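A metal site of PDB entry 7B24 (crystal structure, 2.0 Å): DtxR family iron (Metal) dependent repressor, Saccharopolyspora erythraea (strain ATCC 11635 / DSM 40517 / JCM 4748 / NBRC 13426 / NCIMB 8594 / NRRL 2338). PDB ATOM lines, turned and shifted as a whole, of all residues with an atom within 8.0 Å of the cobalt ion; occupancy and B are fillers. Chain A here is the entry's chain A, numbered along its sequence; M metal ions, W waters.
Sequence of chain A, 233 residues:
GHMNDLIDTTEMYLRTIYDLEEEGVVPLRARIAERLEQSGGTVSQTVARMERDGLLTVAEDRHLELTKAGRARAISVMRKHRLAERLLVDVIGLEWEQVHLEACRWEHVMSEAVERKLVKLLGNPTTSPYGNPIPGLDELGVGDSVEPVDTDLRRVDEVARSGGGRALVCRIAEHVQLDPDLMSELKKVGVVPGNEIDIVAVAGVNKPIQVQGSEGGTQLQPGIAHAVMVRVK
ND1 of His 108 sits at hydrogen-bond distance from OE1 of Glu 11. A ring nitrogen (NE2) of His 108 sits close to the backbone carbonyl oxygen (O) of Leu 6 (3.5 Å). The side-chain sulfur (SG) of Cys 104 lies close to the guanidinium group (NH1) of Arg 15. The side-chain carboxylate of Glu 107 lies within salt-bridge range of the guanidinium group of Arg 15 (3.2 Å). ND1 of His 81 is in hydrogen-bond range of OE1 of Glu 107. OG1 of Thr 16 sits at hydrogen-bond distance from O of Met 12, 2.5 Å away.
The nearest printed residue that does not touch the cobalt ion is Arg 15 (4.1 Å).
The cobalt ion is bound by the backbone carbonyl oxygen (O) of Cys 104 (2.0 Å), the side-chain carboxylate (OE2) of Glu 107 (2.1 Å), a ring nitrogen (NE2) of His 108 (2.3 Å), water W1 (2.3 Å), the side-chain sulfur (SD) of Met 12 (2.4 Å) and the side-chain sulfur (SG) of Cys 104 (2.8 Å). The cobalt ion has six donor atoms within binding distance.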
ATOM      1  N   ASN A   4     -30.899  25.606  10.155  1.00  0.00           N
ATOM      2  CA  ASN A   4     -29.901  24.546   9.808  1.00  0.00           C
ATOM      3  C   ASN A   4     -28.688  24.692  10.744  1.00  0.00           C
ATOM      4  O   ASN A   4     -28.052  25.763  10.718  1.00  0.00           O
ATOM      5  CB  ASN A   4     -29.507  24.615   8.334  1.00  0.00           C
ATOM      6  CG  ASN A   4     -28.966  23.308   7.792  1.00  0.00           C
ATOM      7  OD1 ASN A   4     -29.578  22.251   7.971  1.00  0.00           O
ATOM      8  ND2 ASN A   4     -27.847  23.361   7.088  1.00  0.00           N
ATOM      9  N   ASP A   5     -28.389  23.656  11.538  1.00  0.00           N
ATOM     10  CA  ASP A   5     -27.300  23.644  12.552  1.00  0.00           C
ATOM     11  C   ASP A   5     -25.945  23.711  11.843  1.00  0.00           C
ATOM     12  O   ASP A   5     -25.653  22.805  11.037  1.00  0.00           O
ATOM     13  CB  ASP A   5     -27.390  22.418  13.463  1.00  0.00           C
ATOM     14  CG  ASP A   5     -26.392  22.409  14.612  1.00  0.00           C
ATOM     15  OD1 ASP A   5     -25.908  23.501  14.969  1.00  0.00           O
ATOM     16  OD2 ASP A   5     -26.113  21.319  15.139  1.00  0.00           O
ATOM     17  N   LEU A   6     -25.146  24.730  12.156  1.00  0.00           N
ATOM     18  CA  LEU A   6     -23.825  25.000  11.523  1.00  0.00           C
ATOM     19  C   LEU A   6     -22.769  24.038  12.065  1.00  0.00           C
ATOM     20  O   LEU A   6     -21.691  23.954  11.440  1.00  0.00           O
ATOM     21  CB  LEU A   6     -23.423  26.454  11.798  1.00  0.00           C
ATOM     22  CG  LEU A   6     -24.358  27.522  11.228  1.00  0.00           C
ATOM     23  CD1 LEU A   6     -23.906  28.913  11.659  1.00  0.00           C
ATOM     24  CD2 LEU A   6     -24.446  27.432   9.712  1.00  0.00           C
ATOM     25  N   ILE A   7     -23.046  23.363  13.185  1.00  0.00           N
ATOM     26  CA  ILE A   7     -22.121  22.438  13.906  1.00  0.00           C
ATOM     27  C   ILE A   7     -21.009  23.271  14.558  1.00  0.00           C
ATOM     28  O   ILE A   7     -20.852  23.176  15.788  1.00  0.00           O
ATOM     29  CB  ILE A   7     -21.541  21.345  12.971  1.00  0.00           C
ATOM     30  CG1 ILE A   7     -22.628  20.660  12.131  1.00  0.00           C
ATOM     31  CG2 ILE A   7     -20.733  20.339  13.773  1.00  0.00           C
ATOM     32  CD1 ILE A   7     -23.685  19.948  12.941  1.00  0.00           C
ATOM     33  N   ASP A   8     -20.272  24.046  13.757  1.00  0.00           N
ATOM     34  CA  ASP A   8     -19.202  24.975  14.208  1.00  0.00           C
ATOM     35  C   ASP A   8     -19.404  26.335  13.509  1.00  0.00           C
ATOM     36  O   ASP A   8     -19.164  26.414  12.296  1.00  0.00           O
ATOM     37  CB  ASP A   8     -17.815  24.392  13.946  1.00  0.00           C
ATOM     38  CG  ASP A   8     -16.668  25.162  14.568  1.00  0.00           C
ATOM     39  OD1 ASP A   8     -16.605  26.387  14.366  1.00  0.00           O
ATOM     40  OD2 ASP A   8     -15.845  24.524  15.265  1.00  0.00           O
ATOM     41  N   GLU A  11     -16.038  28.014  11.914  1.00  0.00           N
ATOM     42  CA  GLU A  11     -15.589  27.304  10.695  1.00  0.00           C
ATOM     43  C   GLU A  11     -16.524  27.641   9.525  1.00  0.00           C
ATOM     44  O   GLU A  11     -16.027  27.771   8.389  1.00  0.00           O
ATOM     45  CB  GLU A  11     -15.486  25.802  10.948  1.00  0.00           C
ATOM     46  CG  GLU A  11     -14.332  25.444  11.877  1.00  0.00           C
ATOM     47  CD  GLU A  11     -14.048  23.972  12.075  1.00  0.00           C
ATOM     48  OE1 GLU A  11     -14.790  23.129  11.528  1.00  0.00           O
ATOM     49  OE2 GLU A  11     -13.066  23.660  12.774  1.00  0.00           O
ATOM     50  N   MET A  12     -17.825  27.810   9.790  1.00  0.00           N
ATOM     51  CA  MET A  12     -18.846  28.085   8.745  1.00  0.00           C
ATOM     52  C   MET A  12     -18.760  29.546   8.285  1.00  0.00           C
ATOM     53  O   MET A  12     -19.064  29.811   7.106  1.00  0.00           O
ATOM     54  CB  MET A  12     -20.260  27.765   9.232  1.00  0.00           C
ATOM     55  CG  MET A  12     -20.594  26.282   9.148  1.00  0.00           C
ATOM     56  SD  MET A  12     -20.194  25.543   7.544  1.00  0.00           S
ATOM     57  CE  MET A  12     -21.261  26.496   6.453  1.00  0.00           C
ATOM     58  N   TYR A  13     -18.364  30.469   9.172  1.00  0.00           N
ATOM     59  CA  TYR A  13     -18.085  31.891   8.829  1.00  0.00           C
ATOM     60  C   TYR A  13     -16.840  31.967   7.935  1.00  0.00           C
ATOM     61  O   TYR A  13     -16.893  32.648   6.896  1.00  0.00           O
ATOM     62  CB  TYR A  13     -17.944  32.754  10.085  1.00  0.00           C
ATOM     63  CG  TYR A  13     -19.237  33.346  10.579  1.00  0.00           C
ATOM     64  CD1 TYR A  13     -20.352  32.556  10.819  1.00  0.00           C
ATOM     65  CD2 TYR A  13     -19.362  34.713  10.803  1.00  0.00           C
ATOM     66  CE1 TYR A  13     -21.548  33.085  11.267  1.00  0.00           C
ATOM     67  CE2 TYR A  13     -20.553  35.264  11.249  1.00  0.00           C
ATOM     68  CZ  TYR A  13     -21.645  34.446  11.482  1.00  0.00           C
ATOM     69  OH  TYR A  13     -22.825  34.968  11.927  1.00  0.00           O
ATOM     70  N   ARG A  15     -15.444  29.562   6.064  1.00  0.00           N
ATOM     71  CA  ARG A  15     -15.672  28.868   4.764  1.00  0.00           C
ATOM     72  C   ARG A  15     -16.601  29.706   3.877  1.00  0.00           C
ATOM     73  O   ARG A  15     -16.411  29.676   2.657  1.00  0.00           O
ATOM     74  CB  ARG A  15     -16.225  27.451   4.969  1.00  0.00           C
ATOM     75  CG  ARG A  15     -15.729  26.450   3.938  1.00  0.00           C
ATOM     76  CD  ARG A  15     -16.720  25.327   3.685  1.00  0.00           C
ATOM     77  NE  ARG A  15     -17.822  25.777   2.855  1.00  0.00           N
ATOM     78  CZ  ARG A  15     -19.024  25.203   2.789  1.00  0.00           C
ATOM     79  NH1 ARG A  15     -19.303  24.139   3.522  1.00  0.00           N
ATOM     80  NH2 ARG A  15     -19.946  25.702   1.978  1.00  0.00           N
ATOM     81  N   THR A  16     -17.552  30.422   4.486  1.00  0.00           N
ATOM     82  CA  THR A  16     -18.512  31.317   3.764  1.00  0.00           C
ATOM     83  C   THR A  16     -17.729  32.462   3.118  1.00  0.00           C
ATOM     84  O   THR A  16     -17.970  32.727   1.922  1.00  0.00           O
ATOM     85  CB  THR A  16     -19.627  31.810   4.688  1.00  0.00           C
ATOM     86  OG1 THR A  16     -20.379  30.668   5.115  1.00  0.00           O
ATOM     87  CG2 THR A  16     -20.554  32.803   4.022  1.00  0.00           C
ATOM     88  N   LEU A  36     -26.093  32.142   5.430  1.00  0.00           N
ATOM     89  CA  LEU A  36     -26.239  31.339   6.673  1.00  0.00           C
ATOM     90  C   LEU A  36     -27.601  31.594   7.320  1.00  0.00           C
ATOM     91  O   LEU A  36     -27.909  30.913   8.325  1.00  0.00           O
ATOM     92  CB  LEU A  36     -25.094  31.678   7.638  1.00  0.00           C
ATOM     93  CG  LEU A  36     -23.689  31.347   7.145  1.00  0.00           C
ATOM     94  CD1 LEU A  36     -22.664  31.635   8.228  1.00  0.00           C
ATOM     95  CD2 LEU A  36     -23.589  29.902   6.688  1.00  0.00           C
ATOM     96  N   VAL A  77     -10.688  23.443   6.645  1.00  0.00           N
ATOM     97  CA  VAL A  77     -12.147  23.138   6.587  1.00  0.00           C
ATOM     98  C   VAL A  77     -12.517  22.764   5.141  1.00  0.00           C
ATOM     99  O   VAL A  77     -13.241  21.767   4.959  1.00  0.00           O
ATOM    100  CB  VAL A  77     -13.028  24.291   7.096  1.00  0.00           C
ATOM    101  CG1 VAL A  77     -14.508  24.041   6.820  1.00  0.00           C
ATOM    102  CG2 VAL A  77     -12.810  24.573   8.576  1.00  0.00           C
ATOM    103  N   HIS A  81     -13.841  19.280   3.604  1.00  0.00           N
ATOM    104  CA  HIS A  81     -15.129  19.356   2.856  1.00  0.00           C
ATOM    105  C   HIS A  81     -15.026  18.604   1.517  1.00  0.00           C
ATOM    106  O   HIS A  81     -15.909  17.761   1.261  1.00  0.00           O
ATOM    107  CB  HIS A  81     -15.527  20.819   2.607  1.00  0.00           C
ATOM    108  CG  HIS A  81     -16.833  20.957   1.907  1.00  0.00           C
ATOM    109  ND1 HIS A  81     -18.038  20.706   2.546  1.00  0.00           N
ATOM    110  CD2 HIS A  81     -17.131  21.282   0.632  1.00  0.00           C
ATOM    111  CE1 HIS A  81     -19.026  20.899   1.685  1.00  0.00           C
ATOM    112  NE2 HIS A  81     -18.498  21.248   0.508  1.00  0.00           N
ATOM    113  N   HIS A 100     -23.067  17.457  -0.908  1.00  0.00           N
ATOM    114  CA  HIS A 100     -22.594  18.743  -0.329  1.00  0.00           C
ATOM    115  C   HIS A 100     -23.136  18.932   1.093  1.00  0.00           C
ATOM    116  O   HIS A 100     -22.327  19.286   1.978  1.00  0.00           O
ATOM    117  CB  HIS A 100     -22.954  19.940  -1.221  1.00  0.00           C
ATOM    118  CG  HIS A 100     -22.641  21.247  -0.575  1.00  0.00           C
ATOM    119  ND1 HIS A 100     -21.369  21.781  -0.560  1.00  0.00           N
ATOM    120  CD2 HIS A 100     -23.423  22.117   0.100  1.00  0.00           C
ATOM    121  CE1 HIS A 100     -21.383  22.924   0.083  1.00  0.00           C
ATOM    122  NE2 HIS A 100     -22.634  23.157   0.505  1.00  0.00           N
ATOM    123  N   LEU A 101     -24.438  18.723   1.292  1.00  0.00           N
ATOM    124  CA  LEU A 101     -25.130  18.921   2.599  1.00  0.00           C
ATOM    125  C   LEU A 101     -24.493  17.990   3.644  1.00  0.00           C
ATOM    126  O   LEU A 101     -24.345  18.426   4.802  1.00  0.00           O
ATOM    127  CB  LEU A 101     -26.628  18.637   2.453  1.00  0.00           C
ATOM    128  CG  LEU A 101     -27.485  19.101   3.633  1.00  0.00           C
ATOM    129  CD1 LEU A 101     -27.778  20.590   3.550  1.00  0.00           C
ATOM    130  CD2 LEU A 101     -28.784  18.308   3.711  1.00  0.00           C
ATOM    131  N   GLU A 102     -24.154  16.759   3.254  1.00  0.00           N
ATOM    132  CA  GLU A 102     -23.468  15.761   4.121  1.00  0.00           C
ATOM    133  C   GLU A 102     -22.060  16.269   4.436  1.00  0.00           C
ATOM    134  O   GLU A 102     -21.713  16.341   5.640  1.00  0.00           O
ATOM    135  CB  GLU A 102     -23.413  14.394   3.431  1.00  0.00           C
ATOM    136  CG  GLU A 102     -23.132  13.248   4.389  1.00  0.00           C
ATOM    137  CD  GLU A 102     -24.318  12.801   5.234  1.00  0.00           C
ATOM    138  OE1 GLU A 102     -25.464  12.939   4.752  1.00  0.00           O
ATOM    139  OE2 GLU A 102     -24.094  12.311   6.356  1.00  0.00           O
ATOM    140  N   ALA A 103     -21.286  16.621   3.405  1.00  0.00           N
ATOM    141  CA  ALA A 103     -19.884  17.088   3.490  1.00  0.00           C
ATOM    142  C   ALA A 103     -19.788  18.373   4.328  1.00  0.00           C
ATOM    143  O   ALA A 103     -18.732  18.589   4.948  1.00  0.00           O
ATOM    144  CB  ALA A 103     -19.344  17.298   2.095  1.00  0.00           C
ATOM    145  N   CYS A 104     -20.842  19.186   4.354  1.00  0.00           N
ATOM    146  CA  CYS A 104     -20.906  20.473   5.107  1.00  0.00           C
ATOM    147  C   CYS A 104     -20.918  20.209   6.619  1.00  0.00           C
ATOM    148  O   CYS A 104     -20.507  21.111   7.371  1.00  0.00           O
ATOM    149  CB  CYS A 104     -22.122  21.291   4.691  1.00  0.00           C
ATOM    150  SG  CYS A 104     -21.937  23.058   5.063  1.00  0.00           S
ATOM    151  N   ARG A 105     -21.390  19.032   7.058  1.00  0.00           N
ATOM    152  CA  ARG A 105     -21.372  18.615   8.485  1.00  0.00           C
ATOM    153  C   ARG A 105     -20.050  17.897   8.780  1.00  0.00           C
ATOM    154  O   ARG A 105     -19.422  18.213   9.810  1.00  0.00           O
ATOM    155  CB  ARG A 105     -22.570  17.708   8.805  1.00  0.00           C
ATOM    156  CG  ARG A 105     -23.919  18.399   8.713  1.00  0.00           C
ATOM    157  CD  ARG A 105     -25.019  17.600   9.395  1.00  0.00           C
ATOM    158  NE  ARG A 105     -25.141  16.265   8.830  1.00  0.00           N
ATOM    159  CZ  ARG A 105     -25.776  15.962   7.695  1.00  0.00           C
ATOM    160  NH1 ARG A 105     -26.363  16.894   6.973  1.00  0.00           N
ATOM    161  NH2 ARG A 105     -25.813  14.698   7.281  1.00  0.00           N
ATOM    162  N   TRP A 106     -19.635  16.990   7.897  1.00  0.00           N
ATOM    163  CA  TRP A 106     -18.435  16.117   8.037  1.00  0.00           C
ATOM    164  C   TRP A 106     -17.160  16.967   8.161  1.00  0.00           C
ATOM    165  O   TRP A 106     -16.259  16.565   8.914  1.00  0.00           O
ATOM    166  CB  TRP A 106     -18.331  15.134   6.867  1.00  0.00           C
ATOM    167  CG  TRP A 106     -19.284  13.977   6.938  1.00  0.00           C
ATOM    168  CD1 TRP A 106     -20.571  13.986   7.389  1.00  0.00           C
ATOM    169  CD2 TRP A 106     -19.024  12.631   6.506  1.00  0.00           C
ATOM    170  NE1 TRP A 106     -21.128  12.742   7.288  1.00  0.00           N
ATOM    171  CE2 TRP A 106     -20.205  11.890   6.752  1.00  0.00           C
ATOM    172  CE3 TRP A 106     -17.916  11.980   5.958  1.00  0.00           C
ATOM    173  CZ2 TRP A 106     -20.293  10.529   6.463  1.00  0.00           C
ATOM    174  CZ3 TRP A 106     -18.009  10.638   5.663  1.00  0.00           C
ATOM    175  CH2 TRP A 106     -19.181   9.923   5.922  1.00  0.00           C
ATOM    176  N   GLU A 107     -17.086  18.090   7.436  1.00  0.00           N
ATOM    177  CA  GLU A 107     -15.895  18.971   7.351  1.00  0.00           C
ATOM    178  C   GLU A 107     -15.456  19.434   8.749  1.00  0.00           C
ATOM    179  O   GLU A 107     -14.264  19.773   8.901  1.00  0.00           O
ATOM    180  CB  GLU A 107     -16.179  20.176   6.459  1.00  0.00           C
ATOM    181  CG  GLU A 107     -17.253  21.108   6.991  1.00  0.00           C
ATOM    182  CD  GLU A 107     -17.628  22.250   6.068  1.00  0.00           C
ATOM    183  OE1 GLU A 107     -17.129  22.283   4.925  1.00  0.00           O
ATOM    184  OE2 GLU A 107     -18.408  23.118   6.489  1.00  0.00           O
ATOM    185  N   HIS A 108     -16.364  19.461   9.727  1.00  0.00           N
ATOM    186  CA  HIS A 108     -16.134  20.004  11.095  1.00  0.00           C
ATOM    187  C   HIS A 108     -15.658  18.922  12.078  1.00  0.00           C
ATOM    188  O   HIS A 108     -15.307  19.303  13.204  1.00  0.00           O
ATOM    189  CB  HIS A 108     -17.395  20.697  11.621  1.00  0.00           C
ATOM    190  CG  HIS A 108     -17.942  21.722  10.692  1.00  0.00           C
ATOM    191  ND1 HIS A 108     -17.222  22.837  10.310  1.00  0.00           N
ATOM    192  CD2 HIS A 108     -19.128  21.800  10.057  1.00  0.00           C
ATOM    193  CE1 HIS A 108     -17.942  23.560   9.480  1.00  0.00           C
ATOM    194  NE2 HIS A 108     -19.123  22.952   9.307  1.00  0.00           N
HETATM  195 CO    CO M   1     -20.364  23.145   7.340  1.00  0.00          CO
HETATM  196  O   HOH W   1     -22.130  23.341   8.865  1.00  0.00           O
